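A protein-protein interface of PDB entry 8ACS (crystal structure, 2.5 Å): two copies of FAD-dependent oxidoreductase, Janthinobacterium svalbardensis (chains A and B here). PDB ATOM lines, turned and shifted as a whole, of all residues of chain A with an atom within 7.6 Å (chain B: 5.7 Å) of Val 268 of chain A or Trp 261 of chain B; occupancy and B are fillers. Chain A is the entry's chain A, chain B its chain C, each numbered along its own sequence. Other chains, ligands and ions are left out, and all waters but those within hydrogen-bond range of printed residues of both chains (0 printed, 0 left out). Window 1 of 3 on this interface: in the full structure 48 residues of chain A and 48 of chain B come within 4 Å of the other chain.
OE1 of Glu 263 of chain B is in salt-bridge range of NZ of Lys 267 of chain A, at 3.2 Å.
The side-chain carboxylate (OD1) of Asp 260 of chain B is in salt-bridge range of the side-chain amino group (NZ) of Lys 267 of chain A (3.5 Å).
The side-chain carboxylate (OE2) of Glu 270 of chain A is in salt-bridge range of the side-chain amino group (NZ) of Lys 257 of chain B (2.9 Å).
The side-chain amino group (NZ) of Lys 257 of chain B sits at hydrogen-bond distance from the backbone carbonyl oxygen (O) of Val 268 of chain A (3.4 Å).
Glu 263 of chain A touches Met 264 of chain B, but with the chains exchanged Met 264 of chain A does not touch Glu 263 of chain B (6.5 Å).
Met 264 of chain A touches its own counterpart, Met 264 of chain B.
7 positions are printed for both chains.
Of the 14 pairs that touch across the chains among the printed residues, 1 has its exchanged pair printed and touching as well.
Among the printed residues, merely in contact across the chains: Met 264 of chain A with Met 264 of chain B, Trp 167 of chain A with Lys 257 of chain B, Trp 167 of chain A with Asp 260 of chain B, Trp 167 of chain A with Asp 256 of chain B, Val 268 of chain A with Trp 249 of chain B, Glu 263 of chain A with Met 264 of chain B, Val 268 of chain A with Met 264 of chain B, Lys 267 of chain A with Met 264 of chain B, Val 268 of chain A with Trp 261 of chain B and Ile 243 of chain A with Pro 246 of chain B.
NH1 of Arg 203 of chain A is in salt-bridge range of OE1 of Glu 270 of chain A (3.1 Å).
OE2 of Glu 270 of chain A lies within hydrogen-bond range of NE1 of Trp 167 of chain A.
The guanidinium group (NE) of Arg 171 of chain A is in salt-bridge range of the side-chain carboxylate (OE1) of Glu 270 of chain A.
Of the printed residues of chain B, Trp 167 of chain A touches Asp 256, Lys 257 and Asp 260.
Of the printed residues of chain B, Ile 243 of chain A touches Pro 246.
Of the printed residues of chain B, Val 268 of chain A touches Trp 249, Lys 257, Trp 261 and Met 264.
Of the printed residues of chain A, Pro 246 of chain B touches Ile 243 (3.97 Å).
Printed residues of chain A within 4 Å of Asp 256 of chain B: Trp 167.
Trp 261 of chain B touches just one residue of chain A: Val 268 (3.96 Å).
The nearest residue of chain A that does not touch Trp 261 of chain B is Ile 243 of chain A (4.2 Å).
Hydrophobic or aromatic side chains of chain A within 4 Å of the printed part of chain B: Trp 167, Ile 243, Met 264 and Val 268.
Of the 17 printed residues of chain B, 8 touch a printed residue of chain A.
Hydrophobic or aromatic side chains of chain B within 4 Å of the printed part of chain A: Pro 246, Trp 249, Trp 261 and Met 264.
Among the printed residues, 14 pairs touch across the chains.
Among the printed residues, Asp or Glu carboxylates within 4 Å of a Lys or Arg side-chain nitrogen of the other chain: Lys 267 of chain A with Asp 260 of chain B (3.5 Å), Lys 267 of chain A with Glu 263 of chain B (3.2 Å) and Glu 270 of chain A with Lys 257 of chain B (2.9 Å).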
ATOM      1  N   TRP A 167      12.000  18.882   7.020  1.00  0.00           N
ATOM      2  CA  TRP A 167      11.530  17.541   6.701  1.00  0.00           C
ATOM      3  C   TRP A 167      12.695  16.599   6.438  1.00  0.00           C
ATOM      4  O   TRP A 167      12.702  15.453   6.907  1.00  0.00           O
ATOM      5  CB  TRP A 167      10.606  17.605   5.481  1.00  0.00           C
ATOM      6  CG  TRP A 167      10.073  16.288   4.997  1.00  0.00           C
ATOM      7  CD1 TRP A 167       8.931  15.676   5.406  1.00  0.00           C
ATOM      8  CD2 TRP A 167      10.662  15.416   4.007  1.00  0.00           C
ATOM      9  NE1 TRP A 167       8.772  14.469   4.745  1.00  0.00           N
ATOM     10  CE2 TRP A 167       9.818  14.294   3.880  1.00  0.00           C
ATOM     11  CE3 TRP A 167      11.816  15.480   3.219  1.00  0.00           C
ATOM     12  CZ2 TRP A 167      10.077  13.259   2.980  1.00  0.00           C
ATOM     13  CZ3 TRP A 167      12.083  14.433   2.339  1.00  0.00           C
ATOM     14  CH2 TRP A 167      11.215  13.348   2.224  1.00  0.00           C
ATOM     15  N   ARG A 171      13.807  13.225   8.725  1.00  0.00           N
ATOM     16  CA  ARG A 171      13.975  11.922   8.089  1.00  0.00           C
ATOM     17  C   ARG A 171      15.372  11.367   8.349  1.00  0.00           C
ATOM     18  O   ARG A 171      15.529  10.195   8.710  1.00  0.00           O
ATOM     19  CB  ARG A 171      13.702  12.015   6.585  1.00  0.00           C
ATOM     20  CG  ARG A 171      12.317  12.562   6.217  1.00  0.00           C
ATOM     21  CD  ARG A 171      11.202  11.547   6.340  1.00  0.00           C
ATOM     22  NE  ARG A 171      11.523  10.370   5.554  1.00  0.00           N
ATOM     23  CZ  ARG A 171      11.607   9.141   6.046  1.00  0.00           C
ATOM     24  NH1 ARG A 171      11.366   8.892   7.326  1.00  0.00           N
ATOM     25  NH2 ARG A 171      11.931   8.141   5.231  1.00  0.00           N
ATOM     26  N   ARG A 203       3.188   3.274   8.633  1.00  0.00           N
ATOM     27  CA  ARG A 203       3.675   4.657   8.660  1.00  0.00           C
ATOM     28  C   ARG A 203       2.506   5.645   8.715  1.00  0.00           C
ATOM     29  O   ARG A 203       2.553   6.642   9.443  1.00  0.00           O
ATOM     30  CB  ARG A 203       4.609   4.906   7.461  1.00  0.00           C
ATOM     31  CG  ARG A 203       5.016   6.345   7.206  1.00  0.00           C
ATOM     32  CD  ARG A 203       5.702   7.050   8.360  1.00  0.00           C
ATOM     33  NE  ARG A 203       7.072   6.620   8.635  1.00  0.00           N
ATOM     34  CZ  ARG A 203       8.131   7.430   8.624  1.00  0.00           C
ATOM     35  NH1 ARG A 203       8.009   8.733   8.360  1.00  0.00           N
ATOM     36  NH2 ARG A 203       9.341   6.926   8.888  1.00  0.00           N
ATOM     37  N   GLN A 204       1.416   5.335   8.017  1.00  0.00           N
ATOM     38  CA  GLN A 204       0.221   6.156   8.090  1.00  0.00           C
ATOM     39  C   GLN A 204      -0.447   6.142   9.458  1.00  0.00           C
ATOM     40  O   GLN A 204      -1.228   7.046   9.751  1.00  0.00           O
ATOM     41  CB  GLN A 204      -0.775   5.682   7.036  1.00  0.00           C
ATOM     42  CG  GLN A 204      -0.321   6.088   5.668  1.00  0.00           C
ATOM     43  CD  GLN A 204      -0.112   7.578   5.632  1.00  0.00           C
ATOM     44  OE1 GLN A 204      -0.959   8.346   6.107  1.00  0.00           O
ATOM     45  NE2 GLN A 204       1.021   8.001   5.101  1.00  0.00           N
ATOM     46  N   ILE A 243      -1.376   4.726  -3.357  1.00  0.00           N
ATOM     47  CA  ILE A 243      -1.001   5.167  -4.692  1.00  0.00           C
ATOM     48  C   ILE A 243      -1.387   4.072  -5.676  1.00  0.00           C
ATOM     49  O   ILE A 243      -0.640   3.115  -5.876  1.00  0.00           O
ATOM     50  CB  ILE A 243       0.500   5.482  -4.799  1.00  0.00           C
ATOM     51  CG1 ILE A 243       0.932   6.565  -3.820  1.00  0.00           C
ATOM     52  CG2 ILE A 243       0.850   5.874  -6.231  1.00  0.00           C
ATOM     53  CD1 ILE A 243       2.440   6.726  -3.804  1.00  0.00           C
ATOM     54  N   TRP A 261       8.254   0.050  -9.466  1.00  0.00           N
ATOM     55  CA  TRP A 261       7.119   0.641  -8.775  1.00  0.00           C
ATOM     56  C   TRP A 261       7.266   0.490  -7.264  1.00  0.00           C
ATOM     57  O   TRP A 261       7.098   1.459  -6.520  1.00  0.00           O
ATOM     58  CB  TRP A 261       5.830   0.002  -9.266  1.00  0.00           C
ATOM     59  CG  TRP A 261       4.611   0.585  -8.630  1.00  0.00           C
ATOM     60  CD1 TRP A 261       3.934   0.102  -7.554  1.00  0.00           C
ATOM     61  CD2 TRP A 261       3.940   1.775  -9.021  1.00  0.00           C
ATOM     62  NE1 TRP A 261       2.871   0.910  -7.265  1.00  0.00           N
ATOM     63  CE2 TRP A 261       2.855   1.948  -8.152  1.00  0.00           C
ATOM     64  CE3 TRP A 261       4.145   2.711 -10.034  1.00  0.00           C
ATOM     65  CZ2 TRP A 261       1.973   3.011  -8.264  1.00  0.00           C
ATOM     66  CZ3 TRP A 261       3.258   3.763 -10.148  1.00  0.00           C
ATOM     67  CH2 TRP A 261       2.192   3.907  -9.266  1.00  0.00           C
ATOM     68  N   LEU A 262       7.629  -0.711  -6.790  1.00  0.00           N
ATOM     69  CA  LEU A 262       7.818  -0.906  -5.354  1.00  0.00           C
ATOM     70  C   LEU A 262       8.986  -0.075  -4.836  1.00  0.00           C
ATOM     71  O   LEU A 262       8.949   0.420  -3.701  1.00  0.00           O
ATOM     72  CB  LEU A 262       8.015  -2.390  -5.032  1.00  0.00           C
ATOM     73  CG  LEU A 262       6.758  -3.257  -5.160  1.00  0.00           C
ATOM     74  CD1 LEU A 262       7.104  -4.732  -5.031  1.00  0.00           C
ATOM     75  CD2 LEU A 262       5.714  -2.863  -4.132  1.00  0.00           C
ATOM     76  N   GLU A 263      10.035   0.088  -5.647  1.00  0.00           N
ATOM     77  CA  GLU A 263      11.175   0.899  -5.221  1.00  0.00           C
ATOM     78  C   GLU A 263      10.777   2.364  -5.059  1.00  0.00           C
ATOM     79  O   GLU A 263      11.227   3.031  -4.121  1.00  0.00           O
ATOM     80  CB  GLU A 263      12.340   0.788  -6.210  1.00  0.00           C
ATOM     81  CG  GLU A 263      13.610   1.439  -5.685  1.00  0.00           C
ATOM     82  CD  GLU A 263      14.842   1.149  -6.513  1.00  0.00           C
ATOM     83  OE1 GLU A 263      14.708   0.793  -7.706  1.00  0.00           O
ATOM     84  OE2 GLU A 263      15.959   1.265  -5.954  1.00  0.00           O
ATOM     85  N   MET A 264       9.936   2.877  -5.964  1.00  0.00           N
ATOM     86  CA  MET A 264       9.436   4.242  -5.835  1.00  0.00           C
ATOM     87  C   MET A 264       8.450   4.370  -4.689  1.00  0.00           C
ATOM     88  O   MET A 264       8.464   5.365  -3.947  1.00  0.00           O
ATOM     89  CB  MET A 264       8.721   4.664  -7.119  1.00  0.00           C
ATOM     90  CG  MET A 264       7.610   5.703  -6.833  1.00  0.00           C
ATOM     91  SD  MET A 264       6.107   5.683  -7.784  1.00  0.00           S
ATOM     92  CE  MET A 264       5.090   4.580  -6.775  1.00  0.00           C
ATOM     93  N   TYR A 265       7.600   3.358  -4.533  1.00  0.00           N
ATOM     94  CA  TYR A 265       6.564   3.388  -3.518  1.00  0.00           C
ATOM     95  C   TYR A 265       7.165   3.482  -2.136  1.00  0.00           C
ATOM     96  O   TYR A 265       6.697   4.269  -1.295  1.00  0.00           O
ATOM     97  CB  TYR A 265       5.721   2.136  -3.660  1.00  0.00           C
ATOM     98  CG  TYR A 265       4.601   2.034  -2.700  1.00  0.00           C
ATOM     99  CD1 TYR A 265       4.781   1.493  -1.444  1.00  0.00           C
ATOM    100  CD2 TYR A 265       3.361   2.456  -3.055  1.00  0.00           C
ATOM    101  CE1 TYR A 265       3.732   1.382  -0.567  1.00  0.00           C
ATOM    102  CE2 TYR A 265       2.315   2.352  -2.204  1.00  0.00           C
ATOM    103  CZ  TYR A 265       2.497   1.815  -0.964  1.00  0.00           C
ATOM    104  OH  TYR A 265       1.403   1.722  -0.138  1.00  0.00           O
ATOM    105  N   THR A 266       8.220   2.688  -1.900  1.00  0.00           N
ATOM    106  CA  THR A 266       8.912   2.670  -0.620  1.00  0.00           C
ATOM    107  C   THR A 266       9.536   4.026  -0.309  1.00  0.00           C
ATOM    108  O   THR A 266       9.518   4.471   0.843  1.00  0.00           O
ATOM    109  CB  THR A 266       9.980   1.567  -0.634  1.00  0.00           C
ATOM    110  OG1 THR A 266       9.352   0.294  -0.799  1.00  0.00           O
ATOM    111  CG2 THR A 266      10.797   1.567   0.650  1.00  0.00           C
ATOM    112  N   LYS A 267      10.097   4.691  -1.327  1.00  0.00           N
ATOM    113  CA  LYS A 267      10.723   5.998  -1.129  1.00  0.00           C
ATOM    114  C   LYS A 267       9.667   7.038  -0.770  1.00  0.00           C
ATOM    115  O   LYS A 267       9.719   7.634   0.311  1.00  0.00           O
ATOM    116  CB  LYS A 267      11.478   6.391  -2.394  1.00  0.00           C
ATOM    117  CG  LYS A 267      12.278   7.752  -2.397  1.00  0.00           C
ATOM    118  CD  LYS A 267      13.597   7.736  -1.614  1.00  0.00           C
ATOM    119  CE  LYS A 267      14.640   8.785  -2.159  1.00  0.00           C
ATOM    120  NZ  LYS A 267      14.869   8.903  -3.676  1.00  0.00           N
ATOM    121  N   VAL A 268       8.627   7.173  -1.604  1.00  0.00           N
ATOM    122  CA  VAL A 268       7.680   8.274  -1.429  1.00  0.00           C
ATOM    123  C   VAL A 268       6.750   8.045  -0.241  1.00  0.00           C
ATOM    124  O   VAL A 268       6.264   9.019   0.337  1.00  0.00           O
ATOM    125  CB  VAL A 268       6.854   8.520  -2.711  1.00  0.00           C
ATOM    126  CG1 VAL A 268       7.759   8.825  -3.905  1.00  0.00           C
ATOM    127  CG2 VAL A 268       5.913   7.337  -3.009  1.00  0.00           C
ATOM    128  N   MET A 269       6.467   6.785   0.151  1.00  0.00           N
ATOM    129  CA  MET A 269       5.648   6.527   1.343  1.00  0.00           C
ATOM    130  C   MET A 269       6.463   6.499   2.650  1.00  0.00           C
ATOM    131  O   MET A 269       5.899   6.215   3.711  1.00  0.00           O
ATOM    132  CB  MET A 269       4.838   5.231   1.197  1.00  0.00           C
ATOM    133  CG  MET A 269       3.771   5.234   0.113  1.00  0.00           C
ATOM    134  SD  MET A 269       2.815   6.769  -0.005  1.00  0.00           S
ATOM    135  CE  MET A 269       1.779   6.629   1.447  1.00  0.00           C
ATOM    136  N   GLU A 270       7.754   6.832   2.595  1.00  0.00           N
ATOM    137  CA  GLU A 270       8.595   7.082   3.782  1.00  0.00           C
ATOM    138  C   GLU A 270       8.797   5.838   4.652  1.00  0.00           C
ATOM    139  O   GLU A 270       8.852   5.913   5.882  1.00  0.00           O
ATOM    140  CB  GLU A 270       8.050   8.246   4.616  1.00  0.00           C
ATOM    141  CG  GLU A 270       8.008   9.546   3.829  1.00  0.00           C
ATOM    142  CD  GLU A 270       7.732  10.756   4.708  1.00  0.00           C
ATOM    143  OE1 GLU A 270       7.995  10.683   5.927  1.00  0.00           O
ATOM    144  OE2 GLU A 270       7.240  11.784   4.183  1.00  0.00           O
ATOM    145  N   LEU A 271       8.974   4.685   4.014  1.00  0.00           N
ATOM    146  CA  LEU A 271       9.212   3.469   4.773  1.00  0.00           C
ATOM    147  C   LEU A 271      10.633   3.459   5.342  1.00  0.00           C
ATOM    148  O   LEU A 271      11.563   4.047   4.782  1.00  0.00           O
ATOM    149  CB  LEU A 271       8.978   2.245   3.894  1.00  0.00           C
ATOM    150  CG  LEU A 271       7.627   2.189   3.180  1.00  0.00           C
ATOM    151  CD1 LEU A 271       7.364   0.760   2.709  1.00  0.00           C
ATOM    152  CD2 LEU A 271       6.487   2.718   4.041  1.00  0.00           C
ATOM    153  N   MET B 240       1.228  16.200 -10.671  1.00  0.00           N
ATOM    154  CA  MET B 240       1.812  15.899 -11.970  1.00  0.00           C
ATOM    155  C   MET B 240       0.814  15.131 -12.823  1.00  0.00           C
ATOM    156  O   MET B 240      -0.143  14.553 -12.301  1.00  0.00           O
ATOM    157  CB  MET B 240       3.091  15.098 -11.794  1.00  0.00           C
ATOM    158  CG  MET B 240       4.093  15.814 -10.949  1.00  0.00           C
ATOM    159  SD  MET B 240       4.955  17.102 -11.847  1.00  0.00           S
ATOM    160  CE  MET B 240       5.916  16.135 -13.010  1.00  0.00           C
ATOM    161  N   ILE B 243      -0.119  10.572 -12.416  1.00  0.00           N
ATOM    162  CA  ILE B 243      -0.023  10.056 -11.056  1.00  0.00           C
ATOM    163  C   ILE B 243      -0.235  11.184 -10.063  1.00  0.00           C
ATOM    164  O   ILE B 243       0.735  11.826  -9.632  1.00  0.00           O
ATOM    165  CB  ILE B 243       1.317   9.348 -10.810  1.00  0.00           C
ATOM    166  CG1 ILE B 243       1.483   8.197 -11.791  1.00  0.00           C
ATOM    167  CG2 ILE B 243       1.361   8.793  -9.397  1.00  0.00           C
ATOM    168  CD1 ILE B 243       2.822   7.557 -11.733  1.00  0.00           C
ATOM    169  N   PRO B 244      -1.459  11.412  -9.609  1.00  0.00           N
ATOM    170  CA  PRO B 244      -1.691  12.509  -8.666  1.00  0.00           C
ATOM    171  C   PRO B 244      -1.057  12.189  -7.326  1.00  0.00           C
ATOM    172  O   PRO B 244      -0.747  11.037  -7.022  1.00  0.00           O
ATOM    173  CB  PRO B 244      -3.218  12.560  -8.552  1.00  0.00           C
ATOM    174  CG  PRO B 244      -3.648  11.124  -8.768  1.00  0.00           C
ATOM    175  CD  PRO B 244      -2.625  10.517  -9.720  1.00  0.00           C
ATOM    176  N   PHE B 245      -0.838  13.227  -6.520  1.00  0.00           N
ATOM    177  CA  PHE B 245      -0.411  12.952  -5.159  1.00  0.00           C
ATOM    178  C   PHE B 245      -1.500  12.152  -4.440  1.00  0.00           C
ATOM    179  O   PHE B 245      -2.681  12.255  -4.785  1.00  0.00           O
ATOM    180  CB  PHE B 245      -0.098  14.243  -4.419  1.00  0.00           C
ATOM    181  CG  PHE B 245       1.044  15.001  -5.019  1.00  0.00           C
ATOM    182  CD1 PHE B 245       2.355  14.599  -4.785  1.00  0.00           C
ATOM    183  CD2 PHE B 245       0.809  16.072  -5.864  1.00  0.00           C
ATOM    184  CE1 PHE B 245       3.417  15.259  -5.357  1.00  0.00           C
ATOM    185  CE2 PHE B 245       1.859  16.733  -6.444  1.00  0.00           C
ATOM    186  CZ  PHE B 245       3.179  16.328  -6.183  1.00  0.00           C
ATOM    187  N   PRO B 246      -1.123  11.280  -3.507  1.00  0.00           N
ATOM    188  CA  PRO B 246      -2.125  10.501  -2.763  1.00  0.00           C
ATOM    189  C   PRO B 246      -2.858  11.324  -1.704  1.00  0.00           C
ATOM    190  O   PRO B 246      -2.397  12.376  -1.262  1.00  0.00           O
ATOM    191  CB  PRO B 246      -1.281   9.391  -2.114  1.00  0.00           C
ATOM    192  CG  PRO B 246       0.092   9.992  -1.986  1.00  0.00           C
ATOM    193  CD  PRO B 246       0.260  10.868  -3.198  1.00  0.00           C
ATOM    194  N   TRP B 249      -0.948  12.849   1.119  1.00  0.00           N
ATOM    195  CA  TRP B 249       0.169  13.742   0.856  1.00  0.00           C
ATOM    196  C   TRP B 249      -0.061  15.090   1.556  1.00  0.00           C
ATOM    197  O   TRP B 249      -1.208  15.522   1.739  1.00  0.00           O
ATOM    198  CB  TRP B 249       0.325  13.933  -0.653  1.00  0.00           C
ATOM    199  CG  TRP B 249       1.659  14.444  -1.111  1.00  0.00           C
ATOM    200  CD1 TRP B 249       1.965  15.714  -1.455  1.00  0.00           C
ATOM    201  CD2 TRP B 249       2.861  13.680  -1.285  1.00  0.00           C
ATOM    202  NE1 TRP B 249       3.271  15.805  -1.851  1.00  0.00           N
ATOM    203  CE2 TRP B 249       3.850  14.568  -1.756  1.00  0.00           C
ATOM    204  CE3 TRP B 249       3.195  12.335  -1.101  1.00  0.00           C
ATOM    205  CZ2 TRP B 249       5.168  14.156  -2.016  1.00  0.00           C
ATOM    206  CZ3 TRP B 249       4.503  11.921  -1.367  1.00  0.00           C
ATOM    207  CH2 TRP B 249       5.464  12.824  -1.835  1.00  0.00           C
ATOM    208  N   ASP B 256      12.450  18.716  -0.396  1.00  0.00           N
ATOM    209  CA  ASP B 256      13.074  17.417  -0.665  1.00  0.00           C
ATOM    210  C   ASP B 256      12.039  16.326  -0.876  1.00  0.00           C
ATOM    211  O   ASP B 256      12.288  15.376  -1.621  1.00  0.00           O
ATOM    212  CB  ASP B 256      14.026  17.024   0.470  1.00  0.00           C
ATOM    213  CG  ASP B 256      15.230  17.957   0.563  1.00  0.00           C
ATOM    214  OD1 ASP B 256      16.079  17.975  -0.363  1.00  0.00           O
ATOM    215  OD2 ASP B 256      15.290  18.708   1.558  1.00  0.00           O
ATOM    216  N   LYS B 257      10.877  16.441  -0.244  1.00  0.00           N
ATOM    217  CA  LYS B 257       9.813  15.498  -0.546  1.00  0.00           C
ATOM    218  C   LYS B 257       9.334  15.654  -1.992  1.00  0.00           C
ATOM    219  O   LYS B 257       8.997  14.657  -2.641  1.00  0.00           O
ATOM    220  CB  LYS B 257       8.694  15.660   0.486  1.00  0.00           C
ATOM    221  CG  LYS B 257       7.638  14.591   0.442  1.00  0.00           C
ATOM    222  CD  LYS B 257       6.752  14.647   1.682  1.00  0.00           C
ATOM    223  CE  LYS B 257       5.733  13.510   1.686  1.00  0.00           C
ATOM    224  NZ  LYS B 257       6.381  12.218   1.408  1.00  0.00           N
ATOM    225  N   VAL B 258       9.340  16.879  -2.529  1.00  0.00           N
ATOM    226  CA  VAL B 258       9.077  17.069  -3.960  1.00  0.00           C
ATOM    227  C   VAL B 258      10.139  16.376  -4.789  1.00  0.00           C
ATOM    228  O   VAL B 258       9.841  15.742  -5.811  1.00  0.00           O
ATOM    229  CB  VAL B 258       9.016  18.570  -4.306  1.00  0.00           C
ATOM    230  CG1 VAL B 258       8.938  18.777  -5.810  1.00  0.00           C
ATOM    231  CG2 VAL B 258       7.846  19.164  -3.667  1.00  0.00           C
ATOM    232  N   GLY B 259      11.396  16.483  -4.355  1.00  0.00           N
ATOM    233  CA  GLY B 259      12.489  15.879  -5.100  1.00  0.00           C
ATOM    234  C   GLY B 259      12.345  14.381  -5.199  1.00  0.00           C
ATOM    235  O   GLY B 259      12.523  13.801  -6.270  1.00  0.00           O
ATOM    236  N   ASP B 260      12.043  13.738  -4.068  1.00  0.00           N
ATOM    237  CA  ASP B 260      11.800  12.302  -4.045  1.00  0.00           C
ATOM    238  C   ASP B 260      10.693  11.916  -5.003  1.00  0.00           C
ATOM    239  O   ASP B 260      10.839  10.962  -5.779  1.00  0.00           O
ATOM    240  CB  ASP B 260      11.447  11.876  -2.624  1.00  0.00           C
ATOM    241  CG  ASP B 260      12.667  11.740  -1.752  1.00  0.00           C
ATOM    242  OD1 ASP B 260      13.781  11.914  -2.280  1.00  0.00           O
ATOM    243  OD2 ASP B 260      12.511  11.484  -0.547  1.00  0.00           O
ATOM    244  N   TRP B 261       9.604  12.691  -5.000  1.00  0.00           N
ATOM    245  CA  TRP B 261       8.465  12.380  -5.847  1.00  0.00           C
ATOM    246  C   TRP B 261       8.838  12.494  -7.320  1.00  0.00           C
ATOM    247  O   TRP B 261       8.519  11.597  -8.122  1.00  0.00           O
ATOM    248  CB  TRP B 261       7.315  13.319  -5.512  1.00  0.00           C
ATOM    249  CG  TRP B 261       6.121  13.096  -6.334  1.00  0.00           C
ATOM    250  CD1 TRP B 261       5.796  13.734  -7.480  1.00  0.00           C
ATOM    251  CD2 TRP B 261       5.066  12.177  -6.069  1.00  0.00           C
ATOM    252  NE1 TRP B 261       4.603  13.272  -7.958  1.00  0.00           N
ATOM    253  CE2 TRP B 261       4.132  12.311  -7.107  1.00  0.00           C
ATOM    254  CE3 TRP B 261       4.832  11.234  -5.067  1.00  0.00           C
ATOM    255  CZ2 TRP B 261       2.971  11.536  -7.171  1.00  0.00           C
ATOM    256  CZ3 TRP B 261       3.684  10.477  -5.125  1.00  0.00           C
ATOM    257  CH2 TRP B 261       2.762  10.633  -6.164  1.00  0.00           C
ATOM    258  N   LEU B 262       9.548  13.572  -7.686  1.00  0.00           N
ATOM    259  CA  LEU B 262       9.949  13.759  -9.076  1.00  0.00           C
ATOM    260  C   LEU B 262      10.897  12.673  -9.558  1.00  0.00           C
ATOM    261  O   LEU B 262      10.815  12.250 -10.718  1.00  0.00           O
ATOM    262  CB  LEU B 262      10.597  15.127  -9.269  1.00  0.00           C
ATOM    263  CG  LEU B 262       9.587  16.259  -9.281  1.00  0.00           C
ATOM    264  CD1 LEU B 262      10.301  17.602  -9.282  1.00  0.00           C
ATOM    265  CD2 LEU B 262       8.708  16.075 -10.491  1.00  0.00           C
ATOM    266  N   GLU B 263      11.814  12.229  -8.692  1.00  0.00           N
ATOM    267  CA  GLU B 263      12.765  11.183  -9.059  1.00  0.00           C
ATOM    268  C   GLU B 263      12.066   9.866  -9.271  1.00  0.00           C
ATOM    269  O   GLU B 263      12.334   9.155 -10.246  1.00  0.00           O
ATOM    270  CB  GLU B 263      13.805  11.010  -7.967  1.00  0.00           C
ATOM    271  CG  GLU B 263      14.915  10.072  -8.321  1.00  0.00           C
ATOM    272  CD  GLU B 263      16.059  10.162  -7.322  1.00  0.00           C
ATOM    273  OE1 GLU B 263      15.826  10.648  -6.196  1.00  0.00           O
ATOM    274  OE2 GLU B 263      17.191   9.771  -7.669  1.00  0.00           O
ATOM    275  N   MET B 264      11.147   9.545  -8.374  1.00  0.00           N
ATOM    276  CA  MET B 264      10.394   8.320  -8.514  1.00  0.00           C
ATOM    277  C   MET B 264       9.366   8.413  -9.636  1.00  0.00           C
ATOM    278  O   MET B 264       9.129   7.411 -10.326  1.00  0.00           O
ATOM    279  CB  MET B 264       9.812   7.963  -7.160  1.00  0.00           C
ATOM    280  CG  MET B 264      10.886   7.272  -6.203  1.00  0.00           C
ATOM    281  SD  MET B 264      12.511   6.591  -6.804  1.00  0.00           S
ATOM    282  CE  MET B 264      12.196   4.999  -7.598  1.00  0.00           C
ATOM    283  N   TYR B 265       8.762   9.595  -9.848  1.00  0.00           N
ATOM    284  CA  TYR B 265       7.870   9.784 -10.996  1.00  0.00           C
ATOM    285  C   TYR B 265       8.621   9.576 -12.308  1.00  0.00           C
ATOM    286  O   TYR B 265       8.093   8.977 -13.255  1.00  0.00           O
ATOM    287  CB  TYR B 265       7.266  11.183 -10.954  1.00  0.00           C
ATOM    288  CG  TYR B 265       6.324  11.552 -12.078  1.00  0.00           C
ATOM    289  CD1 TYR B 265       6.801  12.057 -13.285  1.00  0.00           C
ATOM    290  CD2 TYR B 265       4.943  11.479 -11.899  1.00  0.00           C
ATOM    291  CE1 TYR B 265       5.924  12.436 -14.303  1.00  0.00           C
ATOM    292  CE2 TYR B 265       4.076  11.851 -12.889  1.00  0.00           C
ATOM    293  CZ  TYR B 265       4.564  12.333 -14.085  1.00  0.00           C
ATOM    294  OH  TYR B 265       3.666  12.685 -15.064  1.00  0.00           O
ATOM    295  N   THR B 266       9.849  10.089 -12.385  1.00  0.00           N
ATOM    296  CA  THR B 266      10.655   9.952 -13.596  1.00  0.00           C
ATOM    297  C   THR B 266      10.962   8.487 -13.905  1.00  0.00           C
ATOM    298  O   THR B 266      10.953   8.077 -15.073  1.00  0.00           O
ATOM    299  CB  THR B 266      11.957  10.757 -13.449  1.00  0.00           C
ATOM    300  OG1 THR B 266      11.660  12.168 -13.317  1.00  0.00           O
ATOM    301  CG2 THR B 266      12.896  10.494 -14.625  1.00  0.00           C
